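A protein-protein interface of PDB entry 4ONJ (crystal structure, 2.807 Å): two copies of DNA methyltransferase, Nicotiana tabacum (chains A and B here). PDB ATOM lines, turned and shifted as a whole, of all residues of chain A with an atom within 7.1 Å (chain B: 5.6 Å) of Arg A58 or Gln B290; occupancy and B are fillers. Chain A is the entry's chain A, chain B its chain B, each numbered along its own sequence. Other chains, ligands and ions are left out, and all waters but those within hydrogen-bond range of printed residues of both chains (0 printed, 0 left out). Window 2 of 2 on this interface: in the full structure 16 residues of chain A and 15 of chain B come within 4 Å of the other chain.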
ATOM      1  N   GLY A  51     -20.526 -12.435  13.464  1.00  0.00           N
ATOM      2  CA  GLY A  51     -19.209 -12.274  12.872  1.00  0.00           C
ATOM      3  C   GLY A  51     -18.207 -13.369  13.190  1.00  0.00           C
ATOM      4  O   GLY A  51     -17.143 -13.436  12.572  1.00  0.00           O
ATOM      5  N   VAL A  52     -18.541 -14.214  14.160  1.00  0.00           N
ATOM      6  CA  VAL A  52     -17.701 -15.344  14.528  1.00  0.00           C
ATOM      7  C   VAL A  52     -17.476 -16.222  13.308  1.00  0.00           C
ATOM      8  O   VAL A  52     -16.343 -16.577  12.985  1.00  0.00           O
ATOM      9  CB  VAL A  52     -18.343 -16.181  15.649  1.00  0.00           C
ATOM     10  CG1 VAL A  52     -17.661 -17.540  15.767  1.00  0.00           C
ATOM     11  CG2 VAL A  52     -18.290 -15.428  16.967  1.00  0.00           C
ATOM     12  N   TRP A  53     -18.562 -16.554  12.620  1.00  0.00           N
ATOM     13  CA  TRP A  53     -18.460 -17.331  11.393  1.00  0.00           C
ATOM     14  C   TRP A  53     -17.795 -16.538  10.271  1.00  0.00           C
ATOM     15  O   TRP A  53     -17.087 -17.110   9.440  1.00  0.00           O
ATOM     16  CB  TRP A  53     -19.826 -17.875  10.965  1.00  0.00           C
ATOM     17  CG  TRP A  53     -20.125 -19.189  11.601  1.00  0.00           C
ATOM     18  CD1 TRP A  53     -21.083 -19.456  12.537  1.00  0.00           C
ATOM     19  CD2 TRP A  53     -19.436 -20.422  11.370  1.00  0.00           C
ATOM     20  NE1 TRP A  53     -21.040 -20.784  12.891  1.00  0.00           N
ATOM     21  CE2 TRP A  53     -20.036 -21.397  12.189  1.00  0.00           C
ATOM     22  CE3 TRP A  53     -18.372 -20.796  10.542  1.00  0.00           C
ATOM     23  CZ2 TRP A  53     -19.608 -22.720  12.207  1.00  0.00           C
ATOM     24  CZ3 TRP A  53     -17.949 -22.109  10.560  1.00  0.00           C
ATOM     25  CH2 TRP A  53     -18.565 -23.055  11.386  1.00  0.00           C
ATOM     26  N   ASP A  54     -18.017 -15.226  10.250  1.00  0.00           N
ATOM     27  CA  ASP A  54     -17.306 -14.366   9.310  1.00  0.00           C
ATOM     28  C   ASP A  54     -15.804 -14.478   9.546  1.00  0.00           C
ATOM     29  O   ASP A  54     -15.036 -14.666   8.605  1.00  0.00           O
ATOM     30  CB  ASP A  54     -17.755 -12.909   9.438  1.00  0.00           C
ATOM     31  CG  ASP A  54     -19.112 -12.658   8.807  1.00  0.00           C
ATOM     32  OD1 ASP A  54     -19.559 -13.495   7.995  1.00  0.00           O
ATOM     33  OD2 ASP A  54     -19.726 -11.613   9.114  1.00  0.00           O
ATOM     34  N   THR A  55     -15.400 -14.381  10.811  1.00  0.00           N
ATOM     35  CA  THR A  55     -13.997 -14.505  11.197  1.00  0.00           C
ATOM     36  C   THR A  55     -13.396 -15.839  10.761  1.00  0.00           C
ATOM     37  O   THR A  55     -12.402 -15.870  10.032  1.00  0.00           O
ATOM     38  CB  THR A  55     -13.817 -14.366  12.723  1.00  0.00           C
ATOM     39  OG1 THR A  55     -14.287 -13.083  13.154  1.00  0.00           O
ATOM     40  CG2 THR A  55     -12.354 -14.522  13.104  1.00  0.00           C
ATOM     41  N   ILE A  56     -14.005 -16.933  11.215  1.00  0.00           N
ATOM     42  CA  ILE A  56     -13.545 -18.284  10.898  1.00  0.00           C
ATOM     43  C   ILE A  56     -13.391 -18.490   9.394  1.00  0.00           C
ATOM     44  O   ILE A  56     -12.410 -19.074   8.931  1.00  0.00           O
ATOM     45  CB  ILE A  56     -14.511 -19.349  11.465  1.00  0.00           C
ATOM     46  CG1 ILE A  56     -14.577 -19.249  12.989  1.00  0.00           C
ATOM     47  CG2 ILE A  56     -14.086 -20.750  11.046  1.00  0.00           C
ATOM     48  CD1 ILE A  56     -15.685 -20.070  13.606  1.00  0.00           C
ATOM     49  N   SER A  57     -14.358 -17.987   8.637  1.00  0.00           N
ATOM     50  CA  SER A  57     -14.333 -18.108   7.186  1.00  0.00           C
ATOM     51  C   SER A  57     -13.178 -17.315   6.568  1.00  0.00           C
ATOM     52  O   SER A  57     -12.459 -17.832   5.713  1.00  0.00           O
ATOM     53  CB  SER A  57     -15.672 -17.663   6.596  1.00  0.00           C
ATOM     54  OG  SER A  57     -15.888 -18.252   5.327  1.00  0.00           O
ATOM     55  N   ARG A  58     -13.000 -16.067   7.009  1.00  0.00           N
ATOM     56  CA  ARG A  58     -11.934 -15.200   6.495  1.00  0.00           C
ATOM     57  C   ARG A  58     -10.552 -15.829   6.635  1.00  0.00           C
ATOM     58  O   ARG A  58      -9.705 -15.693   5.753  1.00  0.00           O
ATOM     59  CB  ARG A  58     -11.929 -13.842   7.210  1.00  0.00           C
ATOM     60  CG  ARG A  58     -13.119 -12.952   6.907  1.00  0.00           C
ATOM     61  CD  ARG A  58     -12.891 -11.518   7.373  1.00  0.00           C
ATOM     62  NE  ARG A  58     -12.519 -11.418   8.784  1.00  0.00           N
ATOM     63  CZ  ARG A  58     -11.334 -10.994   9.216  1.00  0.00           C
ATOM     64  NH1 ARG A  58     -11.083 -10.926  10.516  1.00  0.00           N
ATOM     65  NH2 ARG A  58     -10.397 -10.635   8.347  1.00  0.00           N
ATOM     66  N   PHE A  59     -10.330 -16.513   7.751  1.00  0.00           N
ATOM     67  CA  PHE A  59      -9.035 -17.115   8.029  1.00  0.00           C
ATOM     68  C   PHE A  59      -8.894 -18.486   7.377  1.00  0.00           C
ATOM     69  O   PHE A  59      -7.781 -18.970   7.172  1.00  0.00           O
ATOM     70  CB  PHE A  59      -8.798 -17.202   9.537  1.00  0.00           C
ATOM     71  CG  PHE A  59      -8.455 -15.884  10.171  1.00  0.00           C
ATOM     72  CD1 PHE A  59      -9.437 -14.933  10.402  1.00  0.00           C
ATOM     73  CD2 PHE A  59      -7.152 -15.593  10.532  1.00  0.00           C
ATOM     74  CE1 PHE A  59      -9.123 -13.718  10.982  1.00  0.00           C
ATOM     75  CE2 PHE A  59      -6.835 -14.383  11.114  1.00  0.00           C
ATOM     76  CZ  PHE A  59      -7.822 -13.444  11.338  1.00  0.00           C
ATOM     77  N   LEU A  60     -10.023 -19.107   7.050  1.00  0.00           N
ATOM     78  CA  LEU A  60     -10.006 -20.382   6.343  1.00  0.00           C
ATOM     79  C   LEU A  60     -10.300 -20.213   4.857  1.00  0.00           C
ATOM     80  O   LEU A  60     -11.215 -20.839   4.325  1.00  0.00           O
ATOM     81  CB  LEU A  60     -10.992 -21.373   6.961  1.00  0.00           C
ATOM     82  CG  LEU A  60     -10.434 -22.397   7.955  1.00  0.00           C
ATOM     83  CD1 LEU A  60      -9.021 -22.815   7.579  1.00  0.00           C
ATOM     84  CD2 LEU A  60     -10.478 -21.866   9.367  1.00  0.00           C
ATOM     85  N   TYR A  61      -9.526 -19.350   4.205  1.00  0.00           N
ATOM     86  CA  TYR A  61      -9.549 -19.211   2.750  1.00  0.00           C
ATOM     87  C   TYR A  61     -10.906 -18.802   2.185  1.00  0.00           C
ATOM     88  O   TYR A  61     -11.237 -19.143   1.050  1.00  0.00           O
ATOM     89  CB  TYR A  61      -9.065 -20.506   2.089  1.00  0.00           C
ATOM     90  CG  TYR A  61      -7.818 -21.060   2.734  1.00  0.00           C
ATOM     91  CD1 TYR A  61      -6.595 -20.418   2.586  1.00  0.00           C
ATOM     92  CD2 TYR A  61      -7.863 -22.216   3.501  1.00  0.00           C
ATOM     93  CE1 TYR A  61      -5.452 -20.914   3.178  1.00  0.00           C
ATOM     94  CE2 TYR A  61      -6.723 -22.720   4.099  1.00  0.00           C
ATOM     95  CZ  TYR A  61      -5.520 -22.064   3.933  1.00  0.00           C
ATOM     96  OH  TYR A  61      -4.380 -22.558   4.524  1.00  0.00           O
ATOM     97  N   ASP A  62     -11.679 -18.070   2.982  1.00  0.00           N
ATOM     98  CA  ASP A  62     -12.998 -17.589   2.573  1.00  0.00           C
ATOM     99  C   ASP A  62     -13.902 -18.711   2.070  1.00  0.00           C
ATOM    100  O   ASP A  62     -14.754 -18.497   1.208  1.00  0.00           O
ATOM    101  CB  ASP A  62     -12.878 -16.483   1.519  1.00  0.00           C
ATOM    102  CG  ASP A  62     -12.236 -15.225   2.067  1.00  0.00           C
ATOM    103  OD1 ASP A  62     -12.911 -14.496   2.825  1.00  0.00           O
ATOM    104  OD2 ASP A  62     -11.059 -14.961   1.740  1.00  0.00           O
ATOM    105  N   ILE A  63     -13.703 -19.910   2.605  1.00  0.00           N
ATOM    106  CA  ILE A  63     -14.570 -21.029   2.271  1.00  0.00           C
ATOM    107  C   ILE A  63     -15.876 -20.879   3.042  1.00  0.00           C
ATOM    108  O   ILE A  63     -15.869 -20.521   4.219  1.00  0.00           O
ATOM    109  CB  ILE A  63     -13.929 -22.384   2.622  1.00  0.00           C
ATOM    110  CG1 ILE A  63     -12.563 -22.529   1.957  1.00  0.00           C
ATOM    111  CG2 ILE A  63     -14.821 -23.527   2.185  1.00  0.00           C
ATOM    112  CD1 ILE A  63     -11.927 -23.869   2.199  1.00  0.00           C
ATOM    113  N   ILE A  83     -16.109 -26.429   7.962  1.00  0.00           N
ATOM    114  CA  ILE A  83     -15.322 -25.809   6.906  1.00  0.00           C
ATOM    115  C   ILE A  83     -14.262 -26.783   6.415  1.00  0.00           C
ATOM    116  O   ILE A  83     -13.456 -27.288   7.196  1.00  0.00           O
ATOM    117  CB  ILE A  83     -14.664 -24.505   7.381  1.00  0.00           C
ATOM    118  CG1 ILE A  83     -15.732 -23.558   7.934  1.00  0.00           C
ATOM    119  CG2 ILE A  83     -13.864 -23.867   6.247  1.00  0.00           C
ATOM    120  CD1 ILE A  83     -15.550 -22.111   7.541  1.00  0.00           C
ATOM    121  N   PHE A 338      -8.301 -21.093  17.972  1.00  0.00           N
ATOM    122  CA  PHE A 338      -8.652 -21.192  16.564  1.00  0.00           C
ATOM    123  C   PHE A 338      -7.526 -20.716  15.647  1.00  0.00           C
ATOM    124  O   PHE A 338      -7.310 -21.279  14.575  1.00  0.00           O
ATOM    125  CB  PHE A 338      -9.921 -20.396  16.274  1.00  0.00           C
ATOM    126  CG  PHE A 338     -10.145 -20.142  14.814  1.00  0.00           C
ATOM    127  CD1 PHE A 338     -10.581 -21.162  13.983  1.00  0.00           C
ATOM    128  CD2 PHE A 338      -9.912 -18.890  14.271  1.00  0.00           C
ATOM    129  CE1 PHE A 338     -10.784 -20.933  12.639  1.00  0.00           C
ATOM    130  CE2 PHE A 338     -10.111 -18.656  12.926  1.00  0.00           C
ATOM    131  CZ  PHE A 338     -10.547 -19.677  12.109  1.00  0.00           C
ATOM    132  N   TYR A 339      -6.812 -19.678  16.072  1.00  0.00           N
ATOM    133  CA  TYR A 339      -5.723 -19.136  15.265  1.00  0.00           C
ATOM    134  C   TYR A 339      -4.553 -20.096  15.179  1.00  0.00           C
ATOM    135  O   TYR A 339      -3.764 -20.033  14.237  1.00  0.00           O
ATOM    136  CB  TYR A 339      -5.278 -17.769  15.790  1.00  0.00           C
ATOM    137  CG  TYR A 339      -6.390 -16.754  15.767  1.00  0.00           C
ATOM    138  CD1 TYR A 339      -6.949 -16.347  14.565  1.00  0.00           C
ATOM    139  CD2 TYR A 339      -6.892 -16.214  16.943  1.00  0.00           C
ATOM    140  CE1 TYR A 339      -7.971 -15.430  14.530  1.00  0.00           C
ATOM    141  CE2 TYR A 339      -7.915 -15.292  16.920  1.00  0.00           C
ATOM    142  CZ  TYR A 339      -8.451 -14.902  15.710  1.00  0.00           C
ATOM    143  OH  TYR A 339      -9.470 -13.980  15.679  1.00  0.00           O
ATOM    144  N   ASP B 288      -9.114  -1.331   5.732  1.00  0.00           N
ATOM    145  CA  ASP B 288      -9.217  -2.426   6.672  1.00  0.00           C
ATOM    146  C   ASP B 288      -8.433  -3.611   6.221  1.00  0.00           C
ATOM    147  O   ASP B 288      -8.472  -3.981   5.082  1.00  0.00           O
ATOM    148  CB  ASP B 288     -10.657  -2.790   6.907  1.00  0.00           C
ATOM    149  CG  ASP B 288     -11.037  -2.644   8.332  1.00  0.00           C
ATOM    150  OD1 ASP B 288     -10.497  -3.394   9.158  1.00  0.00           O
ATOM    151  OD2 ASP B 288     -11.855  -1.763   8.634  1.00  0.00           O
ATOM    152  N   VAL B 289      -7.705  -4.205   7.133  1.00  0.00           N
ATOM    153  CA  VAL B 289      -6.902  -5.332   6.778  1.00  0.00           C
ATOM    154  C   VAL B 289      -7.884  -6.373   6.338  1.00  0.00           C
ATOM    155  O   VAL B 289      -7.634  -7.184   5.480  1.00  0.00           O
ATOM    156  CB  VAL B 289      -6.116  -5.816   7.970  1.00  0.00           C
ATOM    157  CG1 VAL B 289      -4.938  -4.917   8.177  1.00  0.00           C
ATOM    158  CG2 VAL B 289      -6.984  -5.759   9.186  1.00  0.00           C
ATOM    159  N   GLN B 290      -9.044  -6.313   6.937  1.00  0.00           N
ATOM    160  CA  GLN B 290     -10.038  -7.322   6.746  1.00  0.00           C
ATOM    161  C   GLN B 290     -10.483  -7.487   5.306  1.00  0.00           C
ATOM    162  O   GLN B 290     -10.851  -8.563   4.912  1.00  0.00           O
ATOM    163  CB  GLN B 290     -11.193  -7.034   7.665  1.00  0.00           C
ATOM    164  CG  GLN B 290     -10.698  -6.561   9.017  1.00  0.00           C
ATOM    165  CD  GLN B 290     -11.664  -6.866  10.141  1.00  0.00           C
ATOM    166  OE1 GLN B 290     -12.824  -7.196   9.901  1.00  0.00           O
ATOM    167  NE2 GLN B 290     -11.193  -6.753  11.374  1.00  0.00           N
ATOM    168  N   GLN B 291     -10.497  -6.423   4.534  1.00  0.00           N
ATOM    169  CA  GLN B 291     -10.935  -6.425   3.146  1.00  0.00           C
ATOM    170  C   GLN B 291      -9.834  -6.971   2.243  1.00  0.00           C
ATOM    171  O   GLN B 291     -10.039  -7.169   1.046  1.00  0.00           O
ATOM    172  CB  GLN B 291     -11.364  -5.023   2.706  1.00  0.00           C
ATOM    173  CG  GLN B 291     -10.406  -3.911   3.106  1.00  0.00           C
ATOM    174  CD  GLN B 291     -10.934  -2.528   2.753  1.00  0.00           C
ATOM    175  OE1 GLN B 291     -10.303  -1.516   3.054  1.00  0.00           O
ATOM    176  NE2 GLN B 291     -12.094  -2.483   2.109  1.00  0.00           N
ATOM    177  N   LEU B 292      -8.663  -7.212   2.826  1.00  0.00           N
ATOM    178  CA  LEU B 292      -7.575  -7.855   2.100  1.00  0.00           C
ATOM    179  C   LEU B 292      -7.683  -9.371   2.201  1.00  0.00           C
ATOM    180  O   LEU B 292      -7.152  -9.989   3.124  1.00  0.00           O
ATOM    181  CB  LEU B 292      -6.208  -7.383   2.603  1.00  0.00           C
ATOM    182  CG  LEU B 292      -5.628  -6.130   1.943  1.00  0.00           C
ATOM    183  CD1 LEU B 292      -4.117  -6.097   2.104  1.00  0.00           C
ATOM    184  CD2 LEU B 292      -6.015  -6.054   0.473  1.00  0.00           C
ATOM    185  N   ASN B 293      -8.384  -9.959   1.239  1.00  0.00           N
ATOM    186  CA  ASN B 293      -8.580 -11.398   1.194  1.00  0.00           C
ATOM    187  C   ASN B 293      -7.775 -12.034   0.070  1.00  0.00           C
ATOM    188  O   ASN B 293      -7.135 -11.335  -0.716  1.00  0.00           O
ATOM    189  CB  ASN B 293     -10.065 -11.717   1.027  1.00  0.00           C
ATOM    190  CG  ASN B 293     -10.695 -10.964  -0.128  1.00  0.00           C
ATOM    191  OD1 ASN B 293     -10.177 -10.967  -1.245  1.00  0.00           O
ATOM    192  ND2 ASN B 293     -11.812 -10.301   0.140  1.00  0.00           N
ATOM    193  N   LEU B 337      -5.895  -8.007  15.621  1.00  0.00           N
ATOM    194  CA  LEU B 337      -5.480  -7.518  14.310  1.00  0.00           C
ATOM    195  C   LEU B 337      -4.144  -8.107  13.872  1.00  0.00           C
ATOM    196  O   LEU B 337      -3.882  -8.239  12.676  1.00  0.00           O
ATOM    197  CB  LEU B 337      -5.418  -5.991  14.293  1.00  0.00           C
ATOM    198  CG  LEU B 337      -6.773  -5.283  14.311  1.00  0.00           C
ATOM    199  CD1 LEU B 337      -6.593  -3.774  14.243  1.00  0.00           C
ATOM    200  CD2 LEU B 337      -7.641  -5.777  13.165  1.00  0.00           C
ATOM    201  N   ASP B 340      -4.461 -10.902  11.640  1.00  0.00           N
ATOM    202  CA  ASP B 340      -4.770 -10.504  10.272  1.00  0.00           C
ATOM    203  C   ASP B 340      -3.496 -10.208   9.484  1.00  0.00           C
ATOM    204  O   ASP B 340      -3.444 -10.426   8.276  1.00  0.00           O
ATOM    205  CB  ASP B 340      -5.719  -9.304  10.241  1.00  0.00           C
ATOM    206  CG  ASP B 340      -7.177  -9.719  10.200  1.00  0.00           C
ATOM    207  OD1 ASP B 340      -7.633 -10.172   9.129  1.00  0.00           O
ATOM    208  OD2 ASP B 340      -7.867  -9.594  11.234  1.00  0.00           O
ATOM    209  N   ARG B 343      -2.112 -13.631   8.762  1.00  0.00           N
ATOM    210  CA  ARG B 343      -2.947 -14.198   7.713  1.00  0.00           C
ATOM    211  C   ARG B 343      -2.530 -13.687   6.347  1.00  0.00           C
ATOM    212  O   ARG B 343      -2.234 -14.472   5.444  1.00  0.00           O
ATOM    213  CB  ARG B 343      -4.419 -13.863   7.938  1.00  0.00           C
ATOM    214  CG  ARG B 343      -5.313 -14.329   6.804  1.00  0.00           C
ATOM    215  CD  ARG B 343      -6.764 -13.981   7.061  1.00  0.00           C
ATOM    216  NE  ARG B 343      -6.943 -12.547   7.250  1.00  0.00           N
ATOM    217  CZ  ARG B 343      -7.074 -11.676   6.257  1.00  0.00           C
ATOM    218  NH1 ARG B 343      -7.043 -12.095   4.998  1.00  0.00           N
ATOM    219  NH2 ARG B 343      -7.233 -10.387   6.520  1.00  0.00           N
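The guanidinium group of Arg A58 lies within salt-bridge range of the side-chain carboxylate of Asp B340.
O of Val B289 lies within hydrogen-bond range of NH2 of Arg B343, at 3.4 Å.
N of Asp A62 sits at hydrogen-bond distance from O of Ser A57, at 2.9 Å.
The backbone carbonyl oxygen (O) of Leu B292 lies within hydrogen-bond range of the guanidinium group (NH1) of Arg B343, 2.8 Å away.
The guanidinium group (NH2) of Arg B343 lies within salt-bridge range of the side-chain carboxylate (OD1) of Asp B340 (2.6 Å).
Arg A58 touches Gln B290 (NH2 to CA, 3.7 Å).
CD of Arg B343 touches O of Arg A58, at 3.6 Å.
OD2 of Asp B340 touches CZ of Phe A59, at 3.9 Å.
CD of Arg B343 touches CD2 of Phe A59, at 3.8 Å.
Asp A62 touches Asn B293 (OD2 to CB, 3.5 Å).
Of chain A, only Arg A58 comes within 4 Å of Gln B290.
Gln B291 touches none of the printed residues of chain A.
Printed residues of chain A within 4 Å of Asp B340: Arg A58 and Phe A59.
Of the printed residues of chain A, Arg B343 touches Arg A58 and Phe A59.
Among the printed residues, Asp or Glu carboxylates within 4 Å of a Lys or Arg side-chain nitrogen of the other chain: Arg A58 with Asp B340.
No position is printed for both chains.
Of the 6 pairs that touch across the chains among the printed residues, none has its exchanged pair printed and touching as well.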
